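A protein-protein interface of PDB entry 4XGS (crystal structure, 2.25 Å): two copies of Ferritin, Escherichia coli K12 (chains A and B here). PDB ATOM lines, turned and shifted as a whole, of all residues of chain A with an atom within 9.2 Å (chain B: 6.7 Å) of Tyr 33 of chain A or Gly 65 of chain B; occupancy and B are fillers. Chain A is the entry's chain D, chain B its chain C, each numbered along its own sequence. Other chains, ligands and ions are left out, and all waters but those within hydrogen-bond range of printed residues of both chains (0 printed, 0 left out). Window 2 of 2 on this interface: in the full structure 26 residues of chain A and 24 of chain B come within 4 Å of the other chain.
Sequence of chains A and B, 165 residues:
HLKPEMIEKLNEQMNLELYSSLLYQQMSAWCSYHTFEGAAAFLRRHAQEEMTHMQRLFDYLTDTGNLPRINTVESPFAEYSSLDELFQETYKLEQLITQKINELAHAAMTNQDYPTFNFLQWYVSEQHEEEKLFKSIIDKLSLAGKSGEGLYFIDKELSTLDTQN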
ATOM      1  N   GLN A  26      -8.299  20.252  -0.586  1.00  0.00           N
ATOM      2  CA  GLN A  26      -7.023  19.976  -1.240  1.00  0.00           C
ATOM      3  C   GLN A  26      -7.050  18.548  -1.861  1.00  0.00           C
ATOM      4  O   GLN A  26      -6.640  18.322  -2.993  1.00  0.00           O
ATOM      5  CB  GLN A  26      -5.900  20.091  -0.259  1.00  0.00           C
ATOM      6  CG  GLN A  26      -4.527  19.975  -0.850  1.00  0.00           C
ATOM      7  CD  GLN A  26      -4.246  21.160  -1.774  1.00  0.00           C
ATOM      8  OE1 GLN A  26      -4.305  22.319  -1.364  1.00  0.00           O
ATOM      9  NE2 GLN A  26      -4.041  20.880  -3.011  1.00  0.00           N
ATOM     10  N   MET A  27      -7.584  17.587  -1.131  1.00  0.00           N
ATOM     11  CA  MET A  27      -7.714  16.227  -1.643  1.00  0.00           C
ATOM     12  C   MET A  27      -8.580  16.196  -2.906  1.00  0.00           C
ATOM     13  O   MET A  27      -8.345  15.391  -3.833  1.00  0.00           O
ATOM     14  CB  MET A  27      -8.361  15.319  -0.595  1.00  0.00           C
ATOM     15  CG  MET A  27      -7.435  14.978   0.566  1.00  0.00           C
ATOM     16  SD  MET A  27      -8.464  14.134   1.741  1.00  0.00           S
ATOM     17  CE  MET A  27      -7.274  13.303   2.754  1.00  0.00           C
ATOM     18  N   SER A  28      -9.551  17.085  -2.980  1.00  0.00           N
ATOM     19  CA  SER A  28     -10.355  17.096  -4.174  1.00  0.00           C
ATOM     20  C   SER A  28      -9.464  17.469  -5.367  1.00  0.00           C
ATOM     21  O   SER A  28      -9.683  16.963  -6.486  1.00  0.00           O
ATOM     22  CB  SER A  28     -11.560  18.050  -4.097  1.00  0.00           C
ATOM     23  OG  SER A  28     -11.133  19.353  -4.431  1.00  0.00           O
ATOM     24  N   ALA A  29      -8.489  18.353  -5.160  1.00  0.00           N
ATOM     25  CA  ALA A  29      -7.579  18.678  -6.273  1.00  0.00           C
ATOM     26  C   ALA A  29      -6.779  17.457  -6.708  1.00  0.00           C
ATOM     27  O   ALA A  29      -6.637  17.234  -7.891  1.00  0.00           O
ATOM     28  CB  ALA A  29      -6.598  19.809  -5.902  1.00  0.00           C
ATOM     29  N   TRP A  30      -6.243  16.683  -5.762  1.00  0.00           N
ATOM     30  CA  TRP A  30      -5.515  15.465  -6.113  1.00  0.00           C
ATOM     31  C   TRP A  30      -6.393  14.599  -6.957  1.00  0.00           C
ATOM     32  O   TRP A  30      -5.958  14.150  -7.983  1.00  0.00           O
ATOM     33  CB  TRP A  30      -5.051  14.703  -4.907  1.00  0.00           C
ATOM     34  CG  TRP A  30      -4.174  13.635  -5.191  1.00  0.00           C
ATOM     35  CD1 TRP A  30      -2.813  13.660  -5.137  1.00  0.00           C
ATOM     36  CD2 TRP A  30      -4.540  12.306  -5.537  1.00  0.00           C
ATOM     37  NE1 TRP A  30      -2.310  12.418  -5.412  1.00  0.00           N
ATOM     38  CE2 TRP A  30      -3.344  11.575  -5.700  1.00  0.00           C
ATOM     39  CE3 TRP A  30      -5.763  11.654  -5.711  1.00  0.00           C
ATOM     40  CZ2 TRP A  30      -3.328  10.214  -6.017  1.00  0.00           C
ATOM     41  CZ3 TRP A  30      -5.757  10.300  -6.085  1.00  0.00           C
ATOM     42  CH2 TRP A  30      -4.539   9.590  -6.239  1.00  0.00           C
ATOM     43  N   CYS A  31      -7.656  14.454  -6.586  1.00  0.00           N
ATOM     44  CA  CYS A  31      -8.505  13.594  -7.309  1.00  0.00           C
ATOM     45  C   CYS A  31      -8.759  14.105  -8.726  1.00  0.00           C
ATOM     46  O   CYS A  31      -8.743  13.270  -9.668  1.00  0.00           O
ATOM     47  CB  CYS A  31      -9.836  13.421  -6.602  1.00  0.00           C
ATOM     48  SG  CYS A  31      -9.740  12.462  -5.087  1.00  0.00           S
ATOM     49  N   SER A  32      -9.079  15.411  -8.874  1.00  0.00           N
ATOM     50  CA  SER A  32      -9.215  16.048 -10.207  1.00  0.00           C
ATOM     51  C   SER A  32      -7.996  15.812 -11.062  1.00  0.00           C
ATOM     52  O   SER A  32      -8.127  15.353 -12.154  1.00  0.00           O
ATOM     53  CB  SER A  32      -9.433  17.550 -10.190  1.00  0.00           C
ATOM     54  OG  SER A  32     -10.620  17.901  -9.558  1.00  0.00           O
ATOM     55  N   TYR A  33      -6.820  16.089 -10.539  1.00  0.00           N
ATOM     56  CA  TYR A  33      -5.580  15.898 -11.284  1.00  0.00           C
ATOM     57  C   TYR A  33      -5.358  14.455 -11.749  1.00  0.00           C
ATOM     58  O   TYR A  33      -4.745  14.224 -12.799  1.00  0.00           O
ATOM     59  CB  TYR A  33      -4.428  16.324 -10.421  1.00  0.00           C
ATOM     60  CG  TYR A  33      -3.080  16.441 -11.107  1.00  0.00           C
ATOM     61  CD1 TYR A  33      -2.799  17.511 -11.972  1.00  0.00           C
ATOM     62  CD2 TYR A  33      -2.061  15.516 -10.854  1.00  0.00           C
ATOM     63  CE1 TYR A  33      -1.560  17.628 -12.588  1.00  0.00           C
ATOM     64  CE2 TYR A  33      -0.814  15.639 -11.463  1.00  0.00           C
ATOM     65  CZ  TYR A  33      -0.584  16.694 -12.321  1.00  0.00           C
ATOM     66  OH  TYR A  33       0.611  16.814 -12.908  1.00  0.00           O
ATOM     67  N   HIS A  34      -5.875  13.484 -10.997  1.00  0.00           N
ATOM     68  CA  HIS A  34      -5.690  12.081 -11.387  1.00  0.00           C
ATOM     69  C   HIS A  34      -6.943  11.503 -12.008  1.00  0.00           C
ATOM     70  O   HIS A  34      -7.036  10.320 -12.122  1.00  0.00           O
ATOM     71  CB  HIS A  34      -5.255  11.236 -10.184  1.00  0.00           C
ATOM     72  CG  HIS A  34      -3.862  11.507  -9.743  1.00  0.00           C
ATOM     73  ND1 HIS A  34      -3.533  12.575  -8.932  1.00  0.00           N
ATOM     74  CD2 HIS A  34      -2.703  10.882 -10.038  1.00  0.00           C
ATOM     75  CE1 HIS A  34      -2.233  12.582  -8.722  1.00  0.00           C
ATOM     76  NE2 HIS A  34      -1.706  11.566  -9.380  1.00  0.00           N
ATOM     77  N   THR A  35      -7.887  12.371 -12.381  1.00  0.00           N
ATOM     78  CA  THR A  35      -9.056  12.067 -13.250  1.00  0.00           C
ATOM     79  C   THR A  35     -10.262  11.480 -12.519  1.00  0.00           C
ATOM     80  O   THR A  35     -11.236  11.126 -13.177  1.00  0.00           O
ATOM     81  CB  THR A  35      -8.715  11.148 -14.463  1.00  0.00           C
ATOM     82  OG1 THR A  35      -8.635   9.812 -14.038  1.00  0.00           O
ATOM     83  CG2 THR A  35      -7.375  11.545 -15.150  1.00  0.00           C
ATOM     84  N   PHE A  36     -10.195  11.398 -11.169  1.00  0.00           N
ATOM     85  CA  PHE A  36     -11.317  10.943 -10.355  1.00  0.00           C
ATOM     86  C   PHE A  36     -12.232  12.112 -10.040  1.00  0.00           C
ATOM     87  O   PHE A  36     -12.267  12.631  -8.932  1.00  0.00           O
ATOM     88  CB  PHE A  36     -10.824  10.221  -9.115  1.00  0.00           C
ATOM     89  CG  PHE A  36      -9.862   9.062  -9.421  1.00  0.00           C
ATOM     90  CD1 PHE A  36     -10.306   7.931 -10.090  1.00  0.00           C
ATOM     91  CD2 PHE A  36      -8.539   9.080  -8.952  1.00  0.00           C
ATOM     92  CE1 PHE A  36      -9.438   6.875 -10.349  1.00  0.00           C
ATOM     93  CE2 PHE A  36      -7.632   8.027  -9.227  1.00  0.00           C
ATOM     94  CZ  PHE A  36      -8.104   6.908  -9.893  1.00  0.00           C
ATOM     95  N   GLU A  37     -13.006  12.491 -11.038  1.00  0.00           N
ATOM     96  CA  GLU A  37     -13.784  13.738 -10.987  1.00  0.00           C
ATOM     97  C   GLU A  37     -14.958  13.541 -10.061  1.00  0.00           C
ATOM     98  O   GLU A  37     -15.407  14.510  -9.397  1.00  0.00           O
ATOM     99  CB  GLU A  37     -14.275  14.237 -12.397  1.00  0.00           C
ATOM    100  CG  GLU A  37     -13.172  14.513 -13.428  1.00  0.00           C
ATOM    101  CD  GLU A  37     -12.231  15.688 -13.109  1.00  0.00           C
ATOM    102  OE1 GLU A  37     -12.560  16.603 -12.299  1.00  0.00           O
ATOM    103  OE2 GLU A  37     -11.124  15.698 -13.696  1.00  0.00           O
ATOM    104  N   ALA A  40     -13.617  13.825  -6.651  1.00  0.00           N
ATOM    105  CA  ALA A  40     -13.333  15.240  -6.472  1.00  0.00           C
ATOM    106  C   ALA A  40     -14.644  16.002  -6.127  1.00  0.00           C
ATOM    107  O   ALA A  40     -14.663  16.805  -5.174  1.00  0.00           O
ATOM    108  CB  ALA A  40     -12.653  15.838  -7.720  1.00  0.00           C
ATOM    109  N   ARG A  44     -15.268  17.966  -2.579  1.00  0.00           N
ATOM    110  CA  ARG A  44     -15.640  19.384  -2.592  1.00  0.00           C
ATOM    111  C   ARG A  44     -16.883  19.629  -1.747  1.00  0.00           C
ATOM    112  O   ARG A  44     -16.922  20.561  -0.958  1.00  0.00           O
ATOM    113  CB  ARG A  44     -15.942  19.842  -4.031  1.00  0.00           C
ATOM    114  CG  ARG A  44     -15.123  20.984  -4.534  1.00  0.00           C
ATOM    115  CD  ARG A  44     -14.685  20.827  -6.004  1.00  0.00           C
ATOM    116  NE  ARG A  44     -15.727  20.317  -6.924  1.00  0.00           N
ATOM    117  CZ  ARG A  44     -15.481  19.501  -7.952  1.00  0.00           C
ATOM    118  NH1 ARG A  44     -16.455  19.092  -8.721  1.00  0.00           N
ATOM    119  NH2 ARG A  44     -14.250  19.082  -8.199  1.00  0.00           N
ATOM    120  N   PHE A  77      -1.495  20.414   1.958  1.00  0.00           N
ATOM    121  CA  PHE A  77      -0.967  19.715   0.776  1.00  0.00           C
ATOM    122  C   PHE A  77      -0.240  18.400   1.116  1.00  0.00           C
ATOM    123  O   PHE A  77       0.538  18.319   2.089  1.00  0.00           O
ATOM    124  CB  PHE A  77      -0.021  20.630  -0.039  1.00  0.00           C
ATOM    125  CG  PHE A  77       0.486  19.972  -1.288  1.00  0.00           C
ATOM    126  CD1 PHE A  77      -0.339  19.868  -2.417  1.00  0.00           C
ATOM    127  CD2 PHE A  77       1.746  19.358  -1.313  1.00  0.00           C
ATOM    128  CE1 PHE A  77       0.111  19.220  -3.575  1.00  0.00           C
ATOM    129  CE2 PHE A  77       2.193  18.700  -2.459  1.00  0.00           C
ATOM    130  CZ  PHE A  77       1.379  18.646  -3.601  1.00  0.00           C
ATOM    131  N   GLU A  79       1.141  14.358  -0.868  1.00  0.00           N
ATOM    132  CA  GLU A  79       1.187  13.396  -1.924  1.00  0.00           C
ATOM    133  C   GLU A  79       0.327  12.186  -1.473  1.00  0.00           C
ATOM    134  O   GLU A  79       0.370  11.806  -0.312  1.00  0.00           O
ATOM    135  CB  GLU A  79       2.642  12.965  -2.117  1.00  0.00           C
ATOM    136  CG  GLU A  79       3.670  14.094  -2.300  1.00  0.00           C
ATOM    137  CD  GLU A  79       3.490  14.901  -3.601  1.00  0.00           C
ATOM    138  OE1 GLU A  79       2.628  14.542  -4.442  1.00  0.00           O
ATOM    139  OE2 GLU A  79       4.222  15.906  -3.794  1.00  0.00           O
ATOM    140  N   TYR A  80      -0.505  11.633  -2.355  1.00  0.00           N
ATOM    141  CA  TYR A  80      -1.142  10.344  -2.111  1.00  0.00           C
ATOM    142  C   TYR A  80      -0.616   9.328  -3.151  1.00  0.00           C
ATOM    143  O   TYR A  80      -0.395   9.670  -4.310  1.00  0.00           O
ATOM    144  CB  TYR A  80      -2.668  10.487  -2.140  1.00  0.00           C
ATOM    145  CG  TYR A  80      -3.106  11.520  -1.151  1.00  0.00           C
ATOM    146  CD1 TYR A  80      -3.169  11.212   0.212  1.00  0.00           C
ATOM    147  CD2 TYR A  80      -3.410  12.820  -1.550  1.00  0.00           C
ATOM    148  CE1 TYR A  80      -3.559  12.174   1.143  1.00  0.00           C
ATOM    149  CE2 TYR A  80      -3.765  13.808  -0.619  1.00  0.00           C
ATOM    150  CZ  TYR A  80      -3.812  13.491   0.732  1.00  0.00           C
ATOM    151  OH  TYR A  80      -4.148  14.423   1.682  1.00  0.00           O
ATOM    152  N   LEU A  86      -5.852   7.897  -0.193  1.00  0.00           N
ATOM    153  CA  LEU A  86      -6.443   9.183   0.149  1.00  0.00           C
ATOM    154  C   LEU A  86      -7.680   8.962   1.039  1.00  0.00           C
ATOM    155  O   LEU A  86      -7.831   9.610   2.089  1.00  0.00           O
ATOM    156  CB  LEU A  86      -6.802   9.939  -1.138  1.00  0.00           C
ATOM    157  CG  LEU A  86      -7.475  11.325  -1.056  1.00  0.00           C
ATOM    158  CD1 LEU A  86      -7.171  12.117  -2.308  1.00  0.00           C
ATOM    159  CD2 LEU A  86      -8.985  11.239  -0.945  1.00  0.00           C
ATOM    160  N   HIS B   1      -1.919  23.430 -20.022  1.00  0.00           N
ATOM    161  CA  HIS B   1      -1.031  24.562 -20.423  1.00  0.00           C
ATOM    162  C   HIS B   1      -1.024  25.554 -19.240  1.00  0.00           C
ATOM    163  O   HIS B   1      -1.313  25.148 -18.075  1.00  0.00           O
ATOM    164  CB  HIS B   1      -1.502  25.217 -21.755  1.00  0.00           C
ATOM    165  CG  HIS B   1      -0.401  25.499 -22.741  1.00  0.00           C
ATOM    166  ND1 HIS B   1       0.637  26.378 -22.491  1.00  0.00           N
ATOM    167  CD2 HIS B   1      -0.195  25.024 -23.995  1.00  0.00           C
ATOM    168  CE1 HIS B   1       1.432  26.430 -23.544  1.00  0.00           C
ATOM    169  NE2 HIS B   1       0.952  25.616 -24.470  1.00  0.00           N
ATOM    170  N   TYR B  60     -10.479  26.613 -11.898  1.00  0.00           N
ATOM    171  CA  TYR B  60      -9.786  27.006 -13.141  1.00  0.00           C
ATOM    172  C   TYR B  60      -8.420  26.315 -13.141  1.00  0.00           C
ATOM    173  O   TYR B  60      -7.988  25.738 -14.119  1.00  0.00           O
ATOM    174  CB  TYR B  60      -9.673  28.546 -13.299  1.00  0.00           C
ATOM    175  CG  TYR B  60      -8.965  28.988 -14.596  1.00  0.00           C
ATOM    176  CD1 TYR B  60      -9.568  28.880 -15.816  1.00  0.00           C
ATOM    177  CD2 TYR B  60      -7.718  29.549 -14.578  1.00  0.00           C
ATOM    178  CE1 TYR B  60      -8.921  29.258 -17.003  1.00  0.00           C
ATOM    179  CE2 TYR B  60      -7.092  29.928 -15.772  1.00  0.00           C
ATOM    180  CZ  TYR B  60      -7.721  29.798 -16.982  1.00  0.00           C
ATOM    181  OH  TYR B  60      -7.085  30.162 -18.184  1.00  0.00           O
ATOM    182  N   LEU B  61      -7.749  26.334 -12.026  1.00  0.00           N
ATOM    183  CA  LEU B  61      -6.474  25.673 -12.010  1.00  0.00           C
ATOM    184  C   LEU B  61      -6.620  24.142 -12.305  1.00  0.00           C
ATOM    185  O   LEU B  61      -5.891  23.589 -13.120  1.00  0.00           O
ATOM    186  CB  LEU B  61      -5.838  25.917 -10.641  1.00  0.00           C
ATOM    187  CG  LEU B  61      -5.220  27.331 -10.627  1.00  0.00           C
ATOM    188  CD1 LEU B  61      -4.969  27.861  -9.235  1.00  0.00           C
ATOM    189  CD2 LEU B  61      -3.903  27.364 -11.401  1.00  0.00           C
ATOM    190  N   THR B  62      -7.572  23.465 -11.660  1.00  0.00           N
ATOM    191  CA  THR B  62      -7.708  22.047 -11.876  1.00  0.00           C
ATOM    192  C   THR B  62      -8.137  21.778 -13.292  1.00  0.00           C
ATOM    193  O   THR B  62      -7.600  20.869 -13.924  1.00  0.00           O
ATOM    194  CB  THR B  62      -8.662  21.330 -10.888  1.00  0.00           C
ATOM    195  OG1 THR B  62     -10.009  21.802 -11.025  1.00  0.00           O
ATOM    196  CG2 THR B  62      -8.196  21.575  -9.499  1.00  0.00           C
ATOM    197  N   ASP B  63      -9.067  22.575 -13.802  1.00  0.00           N
ATOM    198  CA  ASP B  63      -9.498  22.415 -15.195  1.00  0.00           C
ATOM    199  C   ASP B  63      -8.448  22.666 -16.229  1.00  0.00           C
ATOM    200  O   ASP B  63      -8.593  22.188 -17.342  1.00  0.00           O
ATOM    201  CB  ASP B  63     -10.695  23.317 -15.531  1.00  0.00           C
ATOM    202  CG  ASP B  63     -11.947  22.837 -14.852  1.00  0.00           C
ATOM    203  OD1 ASP B  63     -11.980  21.687 -14.397  1.00  0.00           O
ATOM    204  OD2 ASP B  63     -12.898  23.579 -14.768  1.00  0.00           O
ATOM    205  N   THR B  64      -7.406  23.424 -15.925  1.00  0.00           N
ATOM    206  CA  THR B  64      -6.319  23.592 -16.913  1.00  0.00           C
ATOM    207  C   THR B  64      -5.195  22.554 -16.714  1.00  0.00           C
ATOM    208  O   THR B  64      -4.108  22.721 -17.230  1.00  0.00           O
ATOM    209  CB  THR B  64      -5.714  25.001 -16.818  1.00  0.00           C
ATOM    210  OG1 THR B  64      -5.285  25.207 -15.475  1.00  0.00           O
ATOM    211  CG2 THR B  64      -6.724  26.071 -17.228  1.00  0.00           C
ATOM    212  N   GLY B  65      -5.436  21.549 -15.895  1.00  0.00           N
ATOM    213  CA  GLY B  65      -4.457  20.473 -15.631  1.00  0.00           C
ATOM    214  C   GLY B  65      -3.437  20.790 -14.569  1.00  0.00           C
ATOM    215  O   GLY B  65      -2.422  20.159 -14.476  1.00  0.00           O
ATOM    216  N   ASN B  66      -3.722  21.748 -13.711  1.00  0.00           N
ATOM    217  CA  ASN B  66      -2.788  22.077 -12.649  1.00  0.00           C
ATOM    218  C   ASN B  66      -3.324  21.603 -11.296  1.00  0.00           C
ATOM    219  O   ASN B  66      -4.406  21.036 -11.192  1.00  0.00           O
ATOM    220  CB  ASN B  66      -2.446  23.551 -12.708  1.00  0.00           C
ATOM    221  CG  ASN B  66      -1.771  23.905 -14.007  1.00  0.00           C
ATOM    222  OD1 ASN B  66      -0.642  23.539 -14.200  1.00  0.00           O
ATOM    223  ND2 ASN B  66      -2.517  24.486 -14.961  1.00  0.00           N
ATOM    224  N   LEU B  67      -2.488  21.690 -10.309  1.00  0.00           N
ATOM    225  CA  LEU B  67      -2.829  21.219  -8.997  1.00  0.00           C
ATOM    226  C   LEU B  67      -2.723  22.451  -8.118  1.00  0.00           C
ATOM    227  O   LEU B  67      -1.638  22.906  -7.812  1.00  0.00           O
ATOM    228  CB  LEU B  67      -1.875  20.130  -8.599  1.00  0.00           C
ATOM    229  CG  LEU B  67      -2.208  19.290  -7.358  1.00  0.00           C
ATOM    230  CD1 LEU B  67      -3.472  18.546  -7.586  1.00  0.00           C
ATOM    231  CD2 LEU B  67      -1.088  18.282  -7.088  1.00  0.00           C
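The backbone carbonyl oxygen of Trp 30 of chain A sits at hydrogen-bond distance from a ring nitrogen (ND1) of His 34 of chain A, 3.0 Å away.
O of Leu 61 of chain B is in hydrogen-bond range of N of Asn 66 of chain B, at 2.9 Å.
The side-chain amide nitrogen of Asn 66 of chain B sits at hydrogen-bond distance from the side-chain hydroxyl of Thr 64 of chain B.
The backbone carbonyl oxygen (O) of Ser 28 of chain A lies within hydrogen-bond range of the side-chain hydroxyl (OG) of Ser 32 of chain A (3.3 Å).
The side-chain amide nitrogen of Asn 66 of chain B lies within hydrogen-bond range of the backbone carbonyl oxygen of His 1 of chain B, at 3.4 Å.
Printed residues of chain B within 4 Å of Trp 30 of chain A: Leu 67 (3.8 Å).
Of chain B, only Gly 65, Asn 66 and Leu 67 come within 4 Å of Tyr 33 of chain A.
No residue of chain A comes within 4 Å of Thr 64 of chain B.
Gly 65 of chain B touches just one residue of chain A: Tyr 33 (3.3 Å).
Of the printed residues of chain A, Leu 67 of chain B touches Ala 29, Trp 30, Tyr 33 and Phe 77.
The nearest residue of chain B that does not touch Tyr 33 of chain A is Thr 62 of chain B (5.6 Å).
The nearest residue of chain A that does not touch Gly 65 of chain B is Ser 32 of chain A (7.2 Å).
The nearest printed residue of chain B that does not touch Ala 29 of chain A is Thr 62 of chain B (4.3 Å).
Leu 67 of chain B touches Ala 29 of chain A (CD1 to O, 3.4 Å).
Trp 30 of chain A touches Leu 67 of chain B (N to CD1, 3.8 Å).
Ser 32 of chain A touches Thr 62 of chain B.
O of Gly 65 of chain B touches CE1 of Tyr 33 of chain A, 3.3 Å away.
O of Asn 66 of chain B touches CD1 of Tyr 33 of chain A, at 3.95 Å.
CB of Tyr 33 of chain A touches CD1 of Leu 67 of chain B (3.7 Å).
CD2 of Leu 67 of chain B touches CE1 of Phe 77 of chain A (3.8 Å).
Printed residues of chain A that touch a printed residue of chain B: Ala 29, Trp 30, Ser 32, Tyr 33 and Phe 77.
Hydrophobic or aromatic side chains of chain A within 4 Å of the printed part of chain B: Ala 29, Tyr 33 and Phe 77.
Along chain A the printed residues that touch a printed residue of chain B span positions 29 to 77.
Among the printed residues, 7 pairs touch across the chains.
No position is printed for both chains.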
